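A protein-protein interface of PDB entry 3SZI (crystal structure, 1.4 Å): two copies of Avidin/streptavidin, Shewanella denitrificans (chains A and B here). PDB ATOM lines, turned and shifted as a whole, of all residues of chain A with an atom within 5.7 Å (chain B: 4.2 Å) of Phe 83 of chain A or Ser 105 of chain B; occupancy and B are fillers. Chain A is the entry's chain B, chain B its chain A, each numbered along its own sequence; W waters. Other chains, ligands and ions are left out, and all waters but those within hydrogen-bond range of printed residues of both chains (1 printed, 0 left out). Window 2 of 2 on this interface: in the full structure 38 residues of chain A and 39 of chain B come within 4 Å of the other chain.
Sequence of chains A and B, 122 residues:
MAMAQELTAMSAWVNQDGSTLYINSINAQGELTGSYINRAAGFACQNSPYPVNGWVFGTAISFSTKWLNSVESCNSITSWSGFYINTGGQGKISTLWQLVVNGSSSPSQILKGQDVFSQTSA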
ATOM      1  N   THR A  59     -20.396   1.658   7.619  1.00  0.00           N
ATOM      2  CA  THR A  59     -21.585   2.475   7.356  1.00  0.00           C
ATOM      3  C   THR A  59     -22.686   1.685   6.624  1.00  0.00           C
ATOM      4  O   THR A  59     -23.783   2.209   6.423  1.00  0.00           O
ATOM      5  CB  THR A  59     -21.273   3.743   6.551  1.00  0.00           C
ATOM      6  OG1 THR A  59     -20.820   3.371   5.247  1.00  0.00           O
ATOM      7  CG2 THR A  59     -20.212   4.605   7.265  1.00  0.00           C
ATOM      8  N   ALA A  60     -22.393   0.451   6.203  1.00  0.00           N
ATOM      9  CA  ALA A  60     -23.449  -0.374   5.577  1.00  0.00           C
ATOM     10  C   ALA A  60     -24.311  -1.026   6.649  1.00  0.00           C
ATOM     11  O   ALA A  60     -23.823  -1.406   7.729  1.00  0.00           O
ATOM     12  CB  ALA A  60     -22.841  -1.411   4.675  1.00  0.00           C
ATOM     13  N   ILE A  61     -25.599  -1.195   6.338  1.00  0.00           N
ATOM     14  CA  ILE A  61     -26.509  -1.783   7.291  1.00  0.00           C
ATOM     15  C   ILE A  61     -27.601  -2.535   6.555  1.00  0.00           C
ATOM     16  O   ILE A  61     -28.047  -2.097   5.513  1.00  0.00           O
ATOM     17  CB  ILE A  61     -27.138  -0.727   8.248  1.00  0.00           C
ATOM     18  CG1 ILE A  61     -28.132  -1.355   9.231  1.00  0.00           C
ATOM     19  CG2 ILE A  61     -27.819   0.419   7.473  1.00  0.00           C
ATOM     20  CD1 ILE A  61     -28.607  -0.405  10.325  1.00  0.00           C
ATOM     21  N   SER A  81     -31.831  -2.596   2.945  1.00  0.00           N
ATOM     22  CA  SER A  81     -30.380  -2.510   2.731  1.00  0.00           C
ATOM     23  C   SER A  81     -30.025  -1.051   2.567  1.00  0.00           C
ATOM     24  O   SER A  81     -30.676  -0.335   1.807  1.00  0.00           O
ATOM     25  CB  SER A  81     -29.969  -3.253   1.462  1.00  0.00           C
ATOM     26  OG  SER A  81     -30.265  -4.637   1.546  1.00  0.00           O
ATOM     27  N   GLY A  82     -29.018  -0.584   3.298  1.00  0.00           N
ATOM     28  CA  GLY A  82     -28.741   0.856   3.241  1.00  0.00           C
ATOM     29  C   GLY A  82     -27.413   1.254   3.820  1.00  0.00           C
ATOM     30  O   GLY A  82     -26.579   0.410   4.174  1.00  0.00           O
ATOM     31  N   PHE A  83     -27.215   2.557   3.900  1.00  0.00           N
ATOM     32  CA  PHE A  83     -25.913   3.064   4.323  1.00  0.00           C
ATOM     33  C   PHE A  83     -26.103   4.353   5.093  1.00  0.00           C
ATOM     34  O   PHE A  83     -27.058   5.090   4.849  1.00  0.00           O
ATOM     35  CB  PHE A  83     -25.013   3.277   3.104  1.00  0.00           C
ATOM     36  CG  PHE A  83     -25.640   4.132   2.040  1.00  0.00           C
ATOM     37  CD1 PHE A  83     -26.320   3.542   0.975  1.00  0.00           C
ATOM     38  CD2 PHE A  83     -25.570   5.526   2.110  1.00  0.00           C
ATOM     39  CE1 PHE A  83     -26.924   4.328  -0.005  1.00  0.00           C
ATOM     40  CE2 PHE A  83     -26.174   6.303   1.143  1.00  0.00           C
ATOM     41  CZ  PHE A  83     -26.835   5.711   0.083  1.00  0.00           C
ATOM     42  N   TYR A  84     -25.221   4.575   6.056  1.00  0.00           N
ATOM     43  CA  TYR A  84     -25.209   5.785   6.860  1.00  0.00           C
ATOM     44  C   TYR A  84     -24.490   6.910   6.132  1.00  0.00           C
ATOM     45  O   TYR A  84     -23.400   6.701   5.585  1.00  0.00           O
ATOM     46  CB  TYR A  84     -24.508   5.511   8.203  1.00  0.00           C
ATOM     47  CG  TYR A  84     -24.368   6.755   9.063  1.00  0.00           C
ATOM     48  CD1 TYR A  84     -25.407   7.156   9.904  1.00  0.00           C
ATOM     49  CD2 TYR A  84     -23.213   7.525   9.022  1.00  0.00           C
ATOM     50  CE1 TYR A  84     -25.309   8.293  10.692  1.00  0.00           C
ATOM     51  CE2 TYR A  84     -23.105   8.669   9.800  1.00  0.00           C
ATOM     52  CZ  TYR A  84     -24.151   9.044  10.635  1.00  0.00           C
ATOM     53  OH  TYR A  84     -24.067  10.180  11.433  1.00  0.00           O
ATOM     54  N   ILE A  85     -25.120   8.085   6.132  1.00  0.00           N
ATOM     55  CA  ILE A  85     -24.492   9.333   5.685  1.00  0.00           C
ATOM     56  C   ILE A  85     -24.831  10.426   6.710  1.00  0.00           C
ATOM     57  O   ILE A  85     -25.869  10.392   7.356  1.00  0.00           O
ATOM     58  CB  ILE A  85     -24.958   9.724   4.252  1.00  0.00           C
ATOM     59  CG2 ILE A  85     -26.481   9.813   4.160  1.00  0.00           C
ATOM     60  N   LYS A  92     -28.218  10.124   8.680  1.00  0.00           N
ATOM     61  CA  LYS A  92     -29.320   9.476   7.952  1.00  0.00           C
ATOM     62  C   LYS A  92     -28.904   8.067   7.546  1.00  0.00           C
ATOM     63  O   LYS A  92     -27.723   7.811   7.285  1.00  0.00           O
ATOM     64  CB  LYS A  92     -29.679  10.251   6.679  1.00  0.00           C
ATOM     65  CG  LYS A  92     -30.191  11.670   6.887  1.00  0.00           C
ATOM     66  CD  LYS A  92     -30.449  12.314   5.543  1.00  0.00           C
ATOM     67  CE  LYS A  92     -31.951  12.495   5.306  1.00  0.00           C
ATOM     68  NZ  LYS A  92     -32.304  12.885   3.883  1.00  0.00           N
ATOM     69  N   ILE A  93     -29.879   7.153   7.461  1.00  0.00           N
ATOM     70  CA  ILE A  93     -29.664   5.860   6.809  1.00  0.00           C
ATOM     71  C   ILE A  93     -30.523   5.849   5.548  1.00  0.00           C
ATOM     72  O   ILE A  93     -31.769   5.942   5.637  1.00  0.00           O
ATOM     73  CB  ILE A  93     -30.049   4.663   7.705  1.00  0.00           C
ATOM     74  CG1 ILE A  93     -29.271   4.718   9.024  1.00  0.00           C
ATOM     75  CG2 ILE A  93     -29.721   3.362   6.995  1.00  0.00           C
ATOM     76  CD1 ILE A  93     -29.791   3.759  10.106  1.00  0.00           C
ATOM     77  N   SER A  94     -29.867   5.755   4.392  1.00  0.00           N
ATOM     78  CA  SER A  94     -30.561   5.738   3.107  1.00  0.00           C
ATOM     79  C   SER A  94     -30.679   4.283   2.684  1.00  0.00           C
ATOM     80  O   SER A  94     -29.675   3.581   2.593  1.00  0.00           O
ATOM     81  CB  SER A  94     -29.809   6.546   2.052  1.00  0.00           C
ATOM     82  OG  SER A  94     -30.534   6.567   0.848  1.00  0.00           O
ATOM     83  N   THR A  95     -31.916   3.839   2.449  1.00  0.00           N
ATOM     84  CA  THR A  95     -32.189   2.425   2.218  1.00  0.00           C
ATOM     85  C   THR A  95     -33.010   2.136   0.971  1.00  0.00           C
ATOM     86  O   THR A  95     -33.788   2.976   0.501  1.00  0.00           O
ATOM     87  CB  THR A  95     -32.971   1.782   3.400  1.00  0.00           C
ATOM     88  OG1 THR A  95     -34.308   2.271   3.423  1.00  0.00           O
ATOM     89  CG2 THR A  95     -32.316   2.049   4.743  1.00  0.00           C
ATOM     90  N   GLY B 103     -19.271   2.148   3.034  1.00  0.00           N
ATOM     91  CA  GLY B 103     -18.769   3.399   2.447  1.00  0.00           C
ATOM     92  C   GLY B 103     -19.617   3.945   1.321  1.00  0.00           C
ATOM     93  O   GLY B 103     -19.271   4.940   0.710  1.00  0.00           O
ATOM     94  N   SER B 104     -20.749   3.310   1.035  1.00  0.00           N
ATOM     95  CA  SER B 104     -21.607   3.771  -0.047  1.00  0.00           C
ATOM     96  C   SER B 104     -22.194   5.145   0.262  1.00  0.00           C
ATOM     97  O   SER B 104     -22.371   5.497   1.424  1.00  0.00           O
ATOM     98  CB  SER B 104     -22.742   2.759  -0.292  1.00  0.00           C
ATOM     99  OG  SER B 104     -22.211   1.575  -0.873  1.00  0.00           O
ATOM    100  N   SER B 105     -22.535   5.890  -0.788  1.00  0.00           N
ATOM    101  CA  SER B 105     -23.076   7.249  -0.662  1.00  0.00           C
ATOM    102  C   SER B 105     -24.332   7.494  -1.503  1.00  0.00           C
ATOM    103  O   SER B 105     -24.956   8.556  -1.382  1.00  0.00           O
ATOM    104  CB  SER B 105     -21.996   8.297  -1.011  1.00  0.00           C
ATOM    105  OG  SER B 105     -21.449   8.038  -2.292  1.00  0.00           O
ATOM    106  N   SER B 106     -24.712   6.522  -2.337  1.00  0.00           N
ATOM    107  CA  SER B 106     -25.888   6.654  -3.200  1.00  0.00           C
ATOM    108  C   SER B 106     -26.630   5.315  -3.313  1.00  0.00           C
ATOM    109  O   SER B 106     -25.976   4.276  -3.400  1.00  0.00           O
ATOM    110  CB  SER B 106     -25.448   7.108  -4.591  1.00  0.00           C
ATOM    111  OG  SER B 106     -26.530   7.034  -5.498  1.00  0.00           O
ATOM    112  N   PRO B 107     -27.989   5.338  -3.345  1.00  0.00           N
ATOM    113  CA  PRO B 107     -28.736   4.070  -3.549  1.00  0.00           C
ATOM    114  C   PRO B 107     -28.371   3.392  -4.867  1.00  0.00           C
ATOM    115  O   PRO B 107     -28.543   2.187  -5.016  1.00  0.00           O
ATOM    116  CB  PRO B 107     -30.199   4.515  -3.599  1.00  0.00           C
ATOM    117  CG  PRO B 107     -30.244   5.862  -2.981  1.00  0.00           C
ATOM    118  CD  PRO B 107     -28.891   6.496  -3.176  1.00  0.00           C
ATOM    119  N   GLN B 109     -25.609   2.634  -5.830  1.00  0.00           N
ATOM    120  CA  GLN B 109     -24.461   1.758  -5.582  1.00  0.00           C
ATOM    121  C   GLN B 109     -24.865   0.419  -4.975  1.00  0.00           C
ATOM    122  O   GLN B 109     -24.039  -0.478  -4.835  1.00  0.00           O
ATOM    123  CB  GLN B 109     -23.461   2.433  -4.653  1.00  0.00           C
ATOM    124  CG  GLN B 109     -22.843   3.716  -5.256  1.00  0.00           C
ATOM    125  CD  GLN B 109     -22.089   4.498  -4.218  1.00  0.00           C
ATOM    126  OE1 GLN B 109     -22.552   4.658  -3.093  1.00  0.00           O
ATOM    127  NE2 GLN B 109     -20.913   4.999  -4.587  1.00  0.00           N
HETATM  128  O   HOH W   1     -21.718   5.470   3.948  1.00  0.00           O
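Water W1 lies within hydrogen-bond range of O of Ser 104 of chain B (2.6 Å), OG1 of Thr 59 of chain A (2.6 Å) and O of Tyr 84 of chain A (2.7 Å).
The side-chain hydroxyl of Thr 59 of chain A is in hydrogen-bond range of the backbone NH of Gly 103 of chain B (3.0 Å).
Among the printed residues, merely in contact across the chains: Phe 83 of chain A with Ser 104 of chain B, Phe 83 of chain A with Ser 105 of chain B, Phe 83 of chain A with Ser 106 of chain B, Phe 83 of chain A with Pro 107 of chain B and Ser 94 of chain A with Pro 107 of chain B.
The side-chain amide oxygen (OE1) of Gln 109 of chain B lies within hydrogen-bond range of the backbone NH (N) of Ser 105 of chain B. The backbone NH (N) of Ser 106 of chain B sits at hydrogen-bond distance from the side-chain amide oxygen (OE1) of Gln 109 of chain B (3.0 Å). O of Phe 83 of chain A lies within hydrogen-bond range of N of Ser 94 of chain A (2.9 Å). The backbone carbonyl oxygen (O) of Thr 59 of chain A lies within hydrogen-bond range of the backbone NH (N) of Tyr 84 of chain A.
Of chain B, only Ser 104, Ser 105, Ser 106 and Pro 107 come within 4 Å of Phe 83 of chain A. Ile 85 of chain A touches none of the printed residues of chain B. Lys 92 of chain A touches none of the printed residues of chain B. Of the printed residues of chain B, Ser 94 of chain A touches Pro 107. Of the printed residues of chain A, Ser 104 of chain B touches Phe 83 (3.3 Å). Ser 105 of chain B touches one residue of chain A. Of the printed residues of chain A, Ser 106 of chain B touches Phe 83. Of the printed residues of chain A, Pro 107 of chain B touches Phe 83 and Ser 94. The nearest printed residue of chain A that does not touch Ser 105 of chain B is Ile 85 of chain A (5.8 Å). The nearest printed residue of chain A that does not touch Pro 107 of chain B is Thr 95 of chain A (5.7 Å).
Printed residues of chain A that touch a printed residue of chain B: Thr 59, Phe 83 and Ser 94. Of the 6 printed residues of chain B, 5 touch a printed residue of chain A. Hydrophobic or aromatic side chains of chain B that line the printed part of chain A: Pro 107. Among the printed residues, no Asp or Glu carboxylate lies within 4 Å of a Lys or Arg side-chain nitrogen of the other chain.
No position is printed for both chains. Of the 6 pairs that touch across the chains among the printed residues, none has its exchanged pair printed and touching as well.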
